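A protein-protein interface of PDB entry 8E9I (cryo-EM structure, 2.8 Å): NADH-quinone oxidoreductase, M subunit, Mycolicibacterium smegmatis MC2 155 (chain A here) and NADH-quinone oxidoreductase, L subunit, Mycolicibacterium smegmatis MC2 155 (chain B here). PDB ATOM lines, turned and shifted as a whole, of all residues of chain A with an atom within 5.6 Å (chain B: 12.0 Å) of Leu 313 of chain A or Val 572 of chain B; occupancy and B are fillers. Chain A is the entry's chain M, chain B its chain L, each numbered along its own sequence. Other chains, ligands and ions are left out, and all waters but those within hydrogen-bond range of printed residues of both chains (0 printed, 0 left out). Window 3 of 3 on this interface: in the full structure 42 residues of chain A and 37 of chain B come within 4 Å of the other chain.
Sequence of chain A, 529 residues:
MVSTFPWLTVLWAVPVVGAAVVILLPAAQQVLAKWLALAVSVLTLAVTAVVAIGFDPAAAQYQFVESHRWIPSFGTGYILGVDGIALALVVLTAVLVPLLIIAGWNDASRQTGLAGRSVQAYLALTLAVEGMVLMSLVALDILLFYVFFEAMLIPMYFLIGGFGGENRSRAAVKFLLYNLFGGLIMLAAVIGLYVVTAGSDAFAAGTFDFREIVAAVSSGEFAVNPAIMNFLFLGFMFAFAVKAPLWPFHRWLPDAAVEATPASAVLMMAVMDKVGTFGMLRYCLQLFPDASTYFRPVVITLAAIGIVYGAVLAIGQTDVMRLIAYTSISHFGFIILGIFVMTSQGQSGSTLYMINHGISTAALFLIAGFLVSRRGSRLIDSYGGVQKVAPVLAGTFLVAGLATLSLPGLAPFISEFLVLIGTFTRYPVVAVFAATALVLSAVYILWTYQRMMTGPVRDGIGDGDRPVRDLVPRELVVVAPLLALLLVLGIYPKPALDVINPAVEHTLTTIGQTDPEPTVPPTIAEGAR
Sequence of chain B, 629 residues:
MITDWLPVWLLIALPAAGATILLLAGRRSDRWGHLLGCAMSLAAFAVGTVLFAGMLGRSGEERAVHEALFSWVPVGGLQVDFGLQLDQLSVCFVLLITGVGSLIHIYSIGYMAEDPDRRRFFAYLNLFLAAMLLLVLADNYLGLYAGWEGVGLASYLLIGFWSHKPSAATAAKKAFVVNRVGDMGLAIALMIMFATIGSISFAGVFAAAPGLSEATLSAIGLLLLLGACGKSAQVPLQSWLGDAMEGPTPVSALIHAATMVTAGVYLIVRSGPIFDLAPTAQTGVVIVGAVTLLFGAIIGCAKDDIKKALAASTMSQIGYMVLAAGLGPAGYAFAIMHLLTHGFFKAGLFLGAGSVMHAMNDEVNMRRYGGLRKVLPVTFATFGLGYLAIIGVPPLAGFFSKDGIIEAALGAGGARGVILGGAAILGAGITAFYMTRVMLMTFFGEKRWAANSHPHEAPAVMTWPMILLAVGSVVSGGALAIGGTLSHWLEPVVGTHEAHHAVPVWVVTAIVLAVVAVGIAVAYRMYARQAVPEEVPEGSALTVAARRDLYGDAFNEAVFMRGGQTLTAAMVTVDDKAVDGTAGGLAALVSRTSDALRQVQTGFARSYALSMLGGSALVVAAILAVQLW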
ATOM      1  N   HIS A 250     -35.277  -3.829  32.849  1.00  0.00           N
ATOM      2  CA  HIS A 250     -34.066  -3.096  33.194  1.00  0.00           C
ATOM      3  C   HIS A 250     -33.623  -2.152  32.087  1.00  0.00           C
ATOM      4  O   HIS A 250     -32.750  -1.308  32.310  1.00  0.00           O
ATOM      5  CB  HIS A 250     -32.948  -4.088  33.466  1.00  0.00           C
ATOM      6  CG  HIS A 250     -32.466  -4.770  32.228  1.00  0.00           C
ATOM      7  ND1 HIS A 250     -33.216  -5.713  31.563  1.00  0.00           N
ATOM      8  CD2 HIS A 250     -31.321  -4.633  31.519  1.00  0.00           C
ATOM      9  CE1 HIS A 250     -32.553  -6.135  30.504  1.00  0.00           C
ATOM     10  NE2 HIS A 250     -31.398  -5.497  30.456  1.00  0.00           N
ATOM     11  N   VAL A 308     -28.229 -13.418  36.905  1.00  0.00           N
ATOM     12  CA  VAL A 308     -27.289 -14.024  35.964  1.00  0.00           C
ATOM     13  C   VAL A 308     -27.200 -13.201  34.684  1.00  0.00           C
ATOM     14  O   VAL A 308     -26.121 -13.031  34.110  1.00  0.00           O
ATOM     15  CB  VAL A 308     -27.682 -15.480  35.663  1.00  0.00           C
ATOM     16  CG1 VAL A 308     -26.837 -16.020  34.527  1.00  0.00           C
ATOM     17  CG2 VAL A 308     -27.506 -16.332  36.900  1.00  0.00           C
ATOM     18  N   TYR A 309     -28.333 -12.685  34.219  1.00  0.00           N
ATOM     19  CA  TYR A 309     -28.398 -11.975  32.950  1.00  0.00           C
ATOM     20  C   TYR A 309     -27.623 -10.667  33.010  1.00  0.00           C
ATOM     21  O   TYR A 309     -26.864 -10.335  32.094  1.00  0.00           O
ATOM     22  CB  TYR A 309     -29.871 -11.743  32.624  1.00  0.00           C
ATOM     23  CG  TYR A 309     -30.195 -10.917  31.410  1.00  0.00           C
ATOM     24  CD1 TYR A 309     -30.268  -9.538  31.486  1.00  0.00           C
ATOM     25  CD2 TYR A 309     -30.501 -11.523  30.205  1.00  0.00           C
ATOM     26  CE1 TYR A 309     -30.599  -8.784  30.385  1.00  0.00           C
ATOM     27  CE2 TYR A 309     -30.828 -10.778  29.096  1.00  0.00           C
ATOM     28  CZ  TYR A 309     -30.877  -9.410  29.191  1.00  0.00           C
ATOM     29  OH  TYR A 309     -31.209  -8.661  28.091  1.00  0.00           O
ATOM     30  N   GLY A 310     -27.803  -9.908  34.088  1.00  0.00           N
ATOM     31  CA  GLY A 310     -27.020  -8.704  34.269  1.00  0.00           C
ATOM     32  C   GLY A 310     -25.544  -9.000  34.414  1.00  0.00           C
ATOM     33  O   GLY A 310     -24.704  -8.273  33.883  1.00  0.00           O
ATOM     34  N   ALA A 311     -25.201 -10.070  35.135  1.00  0.00           N
ATOM     35  CA  ALA A 311     -23.793 -10.439  35.234  1.00  0.00           C
ATOM     36  C   ALA A 311     -23.211 -10.718  33.853  1.00  0.00           C
ATOM     37  O   ALA A 311     -22.147 -10.200  33.495  1.00  0.00           O
ATOM     38  CB  ALA A 311     -23.636 -11.654  36.144  1.00  0.00           C
ATOM     39  N   VAL A 312     -23.922 -11.507  33.048  1.00  0.00           N
ATOM     40  CA  VAL A 312     -23.442 -11.840  31.711  1.00  0.00           C
ATOM     41  C   VAL A 312     -23.295 -10.582  30.869  1.00  0.00           C
ATOM     42  O   VAL A 312     -22.269 -10.374  30.214  1.00  0.00           O
ATOM     43  CB  VAL A 312     -24.390 -12.848  31.037  1.00  0.00           C
ATOM     44  CG1 VAL A 312     -24.043 -12.985  29.571  1.00  0.00           C
ATOM     45  CG2 VAL A 312     -24.325 -14.192  31.733  1.00  0.00           C
ATOM     46  N   LEU A 313     -24.314  -9.724  30.870  1.00  0.00           N
ATOM     47  CA  LEU A 313     -24.245  -8.528  30.040  1.00  0.00           C
ATOM     48  C   LEU A 313     -23.093  -7.633  30.470  1.00  0.00           C
ATOM     49  O   LEU A 313     -22.325  -7.157  29.627  1.00  0.00           O
ATOM     50  CB  LEU A 313     -25.567  -7.766  30.097  1.00  0.00           C
ATOM     51  CG  LEU A 313     -26.717  -8.376  29.297  1.00  0.00           C
ATOM     52  CD1 LEU A 313     -27.886  -7.417  29.259  1.00  0.00           C
ATOM     53  CD2 LEU A 313     -26.292  -8.738  27.883  1.00  0.00           C
ATOM     54  N   ALA A 314     -22.945  -7.407  31.775  1.00  0.00           N
ATOM     55  CA  ALA A 314     -21.783  -6.677  32.260  1.00  0.00           C
ATOM     56  C   ALA A 314     -20.505  -7.295  31.719  1.00  0.00           C
ATOM     57  O   ALA A 314     -19.584  -6.579  31.313  1.00  0.00           O
ATOM     58  CB  ALA A 314     -21.768  -6.666  33.787  1.00  0.00           C
ATOM     59  N   ILE A 315     -20.438  -8.627  31.684  1.00  0.00           N
ATOM     60  CA  ILE A 315     -19.275  -9.271  31.086  1.00  0.00           C
ATOM     61  C   ILE A 315     -19.125  -8.832  29.637  1.00  0.00           C
ATOM     62  O   ILE A 315     -18.021  -8.517  29.177  1.00  0.00           O
ATOM     63  CB  ILE A 315     -19.378 -10.803  31.206  1.00  0.00           C
ATOM     64  CG1 ILE A 315     -19.278 -11.225  32.672  1.00  0.00           C
ATOM     65  CG2 ILE A 315     -18.290 -11.459  30.387  1.00  0.00           C
ATOM     66  CD1 ILE A 315     -19.617 -12.665  32.930  1.00  0.00           C
ATOM     67  N   GLY A 316     -20.234  -8.775  28.905  1.00  0.00           N
ATOM     68  CA  GLY A 316     -20.182  -8.457  27.492  1.00  0.00           C
ATOM     69  C   GLY A 316     -20.057  -6.982  27.176  1.00  0.00           C
ATOM     70  O   GLY A 316     -19.924  -6.635  25.999  1.00  0.00           O
ATOM     71  N   GLN A 317     -20.094  -6.112  28.178  1.00  0.00           N
ATOM     72  CA  GLN A 317     -20.042  -4.681  27.921  1.00  0.00           C
ATOM     73  C   GLN A 317     -18.621  -4.233  27.621  1.00  0.00           C
ATOM     74  O   GLN A 317     -17.683  -4.547  28.359  1.00  0.00           O
ATOM     75  CB  GLN A 317     -20.576  -3.892  29.116  1.00  0.00           C
ATOM     76  CG  GLN A 317     -22.050  -4.087  29.411  1.00  0.00           C
ATOM     77  CD  GLN A 317     -22.889  -4.219  28.166  1.00  0.00           C
ATOM     78  OE1 GLN A 317     -22.878  -3.344  27.304  1.00  0.00           O
ATOM     79  NE2 GLN A 317     -23.634  -5.311  28.068  1.00  0.00           N
ATOM     80  N   TYR A 326     -25.067  -2.702  34.413  1.00  0.00           N
ATOM     81  CA  TYR A 326     -25.564  -4.072  34.403  1.00  0.00           C
ATOM     82  C   TYR A 326     -25.200  -4.802  35.689  1.00  0.00           C
ATOM     83  O   TYR A 326     -25.962  -5.655  36.161  1.00  0.00           O
ATOM     84  CB  TYR A 326     -25.026  -4.819  33.187  1.00  0.00           C
ATOM     85  CG  TYR A 326     -25.781  -4.512  31.921  1.00  0.00           C
ATOM     86  CD1 TYR A 326     -27.131  -4.796  31.812  1.00  0.00           C
ATOM     87  CD2 TYR A 326     -25.140  -3.961  30.825  1.00  0.00           C
ATOM     88  CE1 TYR A 326     -27.824  -4.522  30.659  1.00  0.00           C
ATOM     89  CE2 TYR A 326     -25.825  -3.687  29.663  1.00  0.00           C
ATOM     90  CZ  TYR A 326     -27.166  -3.970  29.586  1.00  0.00           C
ATOM     91  OH  TYR A 326     -27.852  -3.697  28.428  1.00  0.00           O
ATOM     92  N   GLY B 563     -17.497 -21.280  25.129  1.00  0.00           N
ATOM     93  CA  GLY B 563     -18.920 -21.370  25.413  1.00  0.00           C
ATOM     94  C   GLY B 563     -19.426 -20.175  26.195  1.00  0.00           C
ATOM     95  O   GLY B 563     -20.547 -19.707  25.988  1.00  0.00           O
ATOM     96  N   GLY B 564     -18.604 -19.670  27.114  1.00  0.00           N
ATOM     97  CA  GLY B 564     -18.976 -18.465  27.833  1.00  0.00           C
ATOM     98  C   GLY B 564     -19.118 -17.272  26.911  1.00  0.00           C
ATOM     99  O   GLY B 564     -20.040 -16.471  27.055  1.00  0.00           O
ATOM    100  N   GLN B 565     -18.201 -17.133  25.954  1.00  0.00           N
ATOM    101  CA  GLN B 565     -18.316 -16.055  24.979  1.00  0.00           C
ATOM    102  C   GLN B 565     -19.551 -16.241  24.111  1.00  0.00           C
ATOM    103  O   GLN B 565     -20.219 -15.267  23.747  1.00  0.00           O
ATOM    104  CB  GLN B 565     -17.059 -16.000  24.115  1.00  0.00           C
ATOM    105  CG  GLN B 565     -15.832 -15.493  24.845  1.00  0.00           C
ATOM    106  CD  GLN B 565     -14.561 -15.740  24.064  1.00  0.00           C
ATOM    107  OE1 GLN B 565     -14.592 -16.318  22.980  1.00  0.00           O
ATOM    108  NE2 GLN B 565     -13.434 -15.312  24.613  1.00  0.00           N
ATOM    109  N   THR B 566     -19.857 -17.489  23.754  1.00  0.00           N
ATOM    110  CA  THR B 566     -21.080 -17.773  23.013  1.00  0.00           C
ATOM    111  C   THR B 566     -22.300 -17.296  23.786  1.00  0.00           C
ATOM    112  O   THR B 566     -23.165 -16.599  23.245  1.00  0.00           O
ATOM    113  CB  THR B 566     -21.183 -19.273  22.736  1.00  0.00           C
ATOM    114  OG1 THR B 566     -20.009 -19.718  22.052  1.00  0.00           O
ATOM    115  CG2 THR B 566     -22.414 -19.583  21.896  1.00  0.00           C
ATOM    116  N   LEU B 567     -22.378 -17.662  25.064  1.00  0.00           N
ATOM    117  CA  LEU B 567     -23.501 -17.242  25.893  1.00  0.00           C
ATOM    118  C   LEU B 567     -23.546 -15.726  26.022  1.00  0.00           C
ATOM    119  O   LEU B 567     -24.622 -15.123  25.980  1.00  0.00           O
ATOM    120  CB  LEU B 567     -23.398 -17.897  27.269  1.00  0.00           C
ATOM    121  CG  LEU B 567     -24.436 -17.500  28.317  1.00  0.00           C
ATOM    122  CD1 LEU B 567     -25.834 -17.873  27.868  1.00  0.00           C
ATOM    123  CD2 LEU B 567     -24.111 -18.157  29.648  1.00  0.00           C
ATOM    124  N   THR B 568     -22.386 -15.094  26.182  1.00  0.00           N
ATOM    125  CA  THR B 568     -22.335 -13.645  26.314  1.00  0.00           C
ATOM    126  C   THR B 568     -22.887 -12.964  25.073  1.00  0.00           C
ATOM    127  O   THR B 568     -23.744 -12.080  25.168  1.00  0.00           O
ATOM    128  CB  THR B 568     -20.894 -13.200  26.564  1.00  0.00           C
ATOM    129  OG1 THR B 568     -20.414 -13.795  27.776  1.00  0.00           O
ATOM    130  CG2 THR B 568     -20.805 -11.687  26.664  1.00  0.00           C
ATOM    131  N   ALA B 569     -22.395 -13.353  23.898  1.00  0.00           N
ATOM    132  CA  ALA B 569     -22.881 -12.749  22.665  1.00  0.00           C
ATOM    133  C   ALA B 569     -24.361 -13.034  22.467  1.00  0.00           C
ATOM    134  O   ALA B 569     -25.119 -12.156  22.039  1.00  0.00           O
ATOM    135  CB  ALA B 569     -22.072 -13.260  21.476  1.00  0.00           C
ATOM    136  N   ALA B 570     -24.797 -14.253  22.780  1.00  0.00           N
ATOM    137  CA  ALA B 570     -26.206 -14.593  22.638  1.00  0.00           C
ATOM    138  C   ALA B 570     -27.068 -13.706  23.524  1.00  0.00           C
ATOM    139  O   ALA B 570     -28.114 -13.206  23.100  1.00  0.00           O
ATOM    140  CB  ALA B 570     -26.416 -16.069  22.979  1.00  0.00           C
ATOM    141  N   MET B 571     -26.633 -13.486  24.763  1.00  0.00           N
ATOM    142  CA  MET B 571     -27.434 -12.703  25.691  1.00  0.00           C
ATOM    143  C   MET B 571     -27.407 -11.227  25.314  1.00  0.00           C
ATOM    144  O   MET B 571     -28.392 -10.508  25.502  1.00  0.00           O
ATOM    145  CB  MET B 571     -26.932 -12.913  27.118  1.00  0.00           C
ATOM    146  CG  MET B 571     -27.947 -12.542  28.171  1.00  0.00           C
ATOM    147  SD  MET B 571     -29.284 -13.750  28.239  1.00  0.00           S
ATOM    148  CE  MET B 571     -28.796 -14.720  29.662  1.00  0.00           C
ATOM    149  N   VAL B 572     -26.281 -10.755  24.781  1.00  0.00           N
ATOM    150  CA  VAL B 572     -26.182  -9.375  24.313  1.00  0.00           C
ATOM    151  C   VAL B 572     -27.170  -9.183  23.174  1.00  0.00           C
ATOM    152  O   VAL B 572     -27.879  -8.172  23.115  1.00  0.00           O
ATOM    153  CB  VAL B 572     -24.751  -9.025  23.866  1.00  0.00           C
ATOM    154  CG1 VAL B 572     -24.748  -7.753  23.045  1.00  0.00           C
ATOM    155  CG2 VAL B 572     -23.839  -8.871  25.068  1.00  0.00           C
ATOM    156  N   THR B 573     -27.212 -10.147  22.253  1.00  0.00           N
ATOM    157  CA  THR B 573     -28.186 -10.081  21.172  1.00  0.00           C
ATOM    158  C   THR B 573     -29.603 -10.076  21.725  1.00  0.00           C
ATOM    159  O   THR B 573     -30.442  -9.280  21.298  1.00  0.00           O
ATOM    160  CB  THR B 573     -27.997 -11.255  20.212  1.00  0.00           C
ATOM    161  OG1 THR B 573     -26.662 -11.241  19.691  1.00  0.00           O
ATOM    162  CG2 THR B 573     -28.992 -11.179  19.069  1.00  0.00           C
ATOM    163  N   VAL B 574     -29.883 -10.956  22.684  1.00  0.00           N
ATOM    164  CA  VAL B 574     -31.215 -11.006  23.278  1.00  0.00           C
ATOM    165  C   VAL B 574     -31.591  -9.646  23.842  1.00  0.00           C
ATOM    166  O   VAL B 574     -32.682  -9.127  23.580  1.00  0.00           O
ATOM    167  CB  VAL B 574     -31.269 -12.095  24.365  1.00  0.00           C
ATOM    168  CG1 VAL B 574     -32.501 -11.920  25.233  1.00  0.00           C
ATOM    169  CG2 VAL B 574     -31.250 -13.472  23.731  1.00  0.00           C
ATOM    170  N   ASP B 575     -30.692  -9.044  24.616  1.00  0.00           N
ATOM    171  CA  ASP B 575     -30.976  -7.745  25.210  1.00  0.00           C
ATOM    172  C   ASP B 575     -31.251  -6.705  24.135  1.00  0.00           C
ATOM    173  O   ASP B 575     -32.296  -6.045  24.145  1.00  0.00           O
ATOM    174  CB  ASP B 575     -29.799  -7.302  26.076  1.00  0.00           C
ATOM    175  CG  ASP B 575     -30.143  -6.129  26.961  1.00  0.00           C
ATOM    176  OD1 ASP B 575     -30.707  -6.355  28.050  1.00  0.00           O
ATOM    177  OD2 ASP B 575     -29.858  -4.980  26.564  1.00  0.00           O
ATOM    178  N   ASP B 576     -30.332  -6.564  23.182  1.00  0.00           N
ATOM    179  CA  ASP B 576     -30.435  -5.475  22.221  1.00  0.00           C
ATOM    180  C   ASP B 576     -31.593  -5.679  21.257  1.00  0.00           C
ATOM    181  O   ASP B 576     -32.092  -4.708  20.678  1.00  0.00           O
ATOM    182  CB  ASP B 576     -29.126  -5.344  21.448  1.00  0.00           C
ATOM    183  CG  ASP B 576     -27.926  -5.209  22.362  1.00  0.00           C
ATOM    184  OD1 ASP B 576     -26.789  -5.435  21.899  1.00  0.00           O
ATOM    185  OD2 ASP B 576     -28.118  -4.872  23.547  1.00  0.00           O
ATOM    186  N   LYS B 577     -32.040  -6.918  21.079  1.00  0.00           N
ATOM    187  CA  LYS B 577     -32.992  -7.265  20.035  1.00  0.00           C
ATOM    188  C   LYS B 577     -34.342  -7.699  20.576  1.00  0.00           C
ATOM    189  O   LYS B 577     -35.368  -7.433  19.946  1.00  0.00           O
ATOM    190  CB  LYS B 577     -32.407  -8.380  19.158  1.00  0.00           C
ATOM    191  N   ALA B 578     -34.375  -8.384  21.717  1.00  0.00           N
ATOM    192  CA  ALA B 578     -35.640  -8.841  22.281  1.00  0.00           C
ATOM    193  C   ALA B 578     -36.172  -7.867  23.327  1.00  0.00           C
ATOM    194  O   ALA B 578     -37.256  -7.302  23.164  1.00  0.00           O
ATOM    195  CB  ALA B 578     -35.470 -10.238  22.886  1.00  0.00           C
ATOM    196  N   VAL B 579     -35.416  -7.657  24.404  1.00  0.00           N
ATOM    197  CA  VAL B 579     -35.886  -6.779  25.467  1.00  0.00           C
ATOM    198  C   VAL B 579     -36.007  -5.348  24.959  1.00  0.00           C
ATOM    199  O   VAL B 579     -37.053  -4.707  25.102  1.00  0.00           O
ATOM    200  CB  VAL B 579     -34.954  -6.866  26.687  1.00  0.00           C
ATOM    201  CG1 VAL B 579     -35.478  -5.996  27.813  1.00  0.00           C
ATOM    202  CG2 VAL B 579     -34.828  -8.301  27.148  1.00  0.00           C
ATOM    203  N   ASP B 580     -34.946  -4.831  24.344  1.00  0.00           N
ATOM    204  CA  ASP B 580     -35.016  -3.486  23.789  1.00  0.00           C
ATOM    205  C   ASP B 580     -35.912  -3.462  22.561  1.00  0.00           C
ATOM    206  O   ASP B 580     -36.618  -2.479  22.311  1.00  0.00           O
ATOM    207  CB  ASP B 580     -33.619  -2.984  23.438  1.00  0.00           C
ATOM    208  CG  ASP B 580     -33.603  -1.509  23.108  1.00  0.00           C
ATOM    209  OD1 ASP B 580     -34.383  -0.763  23.730  1.00  0.00           O
ATOM    210  OD2 ASP B 580     -32.826  -1.095  22.224  1.00  0.00           O
ATOM    211  N   GLY B 581     -35.882  -4.539  21.776  1.00  0.00           N
ATOM    212  CA  GLY B 581     -36.670  -4.606  20.563  1.00  0.00           C
ATOM    213  C   GLY B 581     -38.160  -4.588  20.800  1.00  0.00           C
ATOM    214  O   GLY B 581     -38.890  -4.011  19.995  1.00  0.00           O
ATOM    215  N   THR B 582     -38.631  -5.206  21.881  1.00  0.00           N
ATOM    216  CA  THR B 582     -40.059  -5.151  22.174  1.00  0.00           C
ATOM    217  C   THR B 582     -40.506  -3.725  22.474  1.00  0.00           C
ATOM    218  O   THR B 582     -41.522  -3.260  21.941  1.00  0.00           O
ATOM    219  CB  THR B 582     -40.391  -6.065  23.353  1.00  0.00           C
ATOM    220  OG1 THR B 582     -39.427  -5.874  24.393  1.00  0.00           O
ATOM    221  CG2 THR B 582     -40.372  -7.523  22.920  1.00  0.00           C
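OD1 of Asp 575 of chain B sits close to OH of Tyr 309 of chain A (2.4 Å). NE2 of His 250 of chain A is in hydrogen-bond range of OD1 of Asp 575 of chain B (2.6 Å). The side-chain carboxylate (OD2) of Asp 575 of chain B sits at hydrogen-bond distance from the side-chain hydroxyl (OH) of Tyr 326 of chain A, 3.0 Å away.
Printed residues of chain B within 4 Å of His 250 of chain A: Asp 575 and Val 579. Printed residues of chain B within 4 Å of Tyr 309 of chain A: Met 571, Asp 575 and Val 579. No residue of chain B comes within 4 Å of Gly 310 of chain A. No residue of chain B comes within 4 Å of Ala 311 of chain A. Val 312 of chain A touches just these residues of chain B: Thr 568 and Met 571. Leu 313 of chain A touches just these residues of chain B: Met 571, Val 572 and Asp 575. No residue of chain B comes within 4 Å of Ala 314 of chain A. No residue of chain B comes within 4 Å of Ile 315 of chain A. Of chain B, only Thr 568 (3.4 Å) comes within 4 Å of Gly 316 of chain A. No residue of chain B comes within 4 Å of Gln 317 of chain A. Tyr 326 of chain A touches just one residue of chain B: Asp 575. Leu 567 of chain B touches none of the printed residues of chain A. Of the printed residues of chain A, Thr 568 of chain B touches Val 312 and Gly 316. Printed residues of chain A within 4 Å of Met 571 of chain B: Tyr 309 (3.2 Å), Val 312 (3.8 Å) and Leu 313 (3.6 Å). Of chain A, only Leu 313 (3.6 Å) comes within 4 Å of Val 572 of chain B. Printed residues of chain A within 4 Å of Asp 575 of chain B: His 250, Tyr 309, Leu 313 and Tyr 326. Printed residues of chain A within 4 Å of Val 579 of chain B: His 250 and Tyr 309. The nearest residue of chain A that does not touch Val 572 of chain B is Gly 316 of chain A (4.4 Å). The nearest printed residue of chain A that does not touch Thr 568 of chain B is Ile 315 of chain A (4.1 Å).
Of the 12 printed residues of chain A, 6 touch a printed residue of chain B. Among the printed residues, no Asp or Glu carboxylate lies within 4 Å of a Lys or Arg side-chain nitrogen of the other chain.
NE2 of Gln 317 of chain A lies within hydrogen-bond range of O of Leu 313 of chain A (2.7 Å). The backbone carbonyl oxygen (O) of Gly 564 of chain B lies within hydrogen-bond range of the side-chain hydroxyl (OG1) of Thr 568 of chain B (2.8 Å). The backbone carbonyl oxygen (O) of Val 579 of chain B is in hydrogen-bond range of the side-chain hydroxyl (OG1) of Thr 582 of chain B (2.7 Å). The backbone carbonyl oxygen (O) of Asp 575 of chain B is in hydrogen-bond range of the backbone NH (N) of Asp 580 of chain B (2.9 Å). N of Val 579 of chain B is in hydrogen-bond range of O of Val 574 of chain B, at 3.2 Å.
Among the printed residues, pairs that only touch across the chains: Tyr 309 of chain A with Met 571 of chain B, Leu 313 of chain A with Asp 575 of chain B, Gly 316 of chain A with Thr 568 of chain B, Leu 313 of chain A with Val 572 of chain B, Leu 313 of chain A with Met 571 of chain B, Val 312 of chain A with Thr 568 of chain B, Tyr 309 of chain A with Val 579 of chain B, Val 312 of chain A with Met 571 of chain B and His 250 of chain A with Val 579 of chain B.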
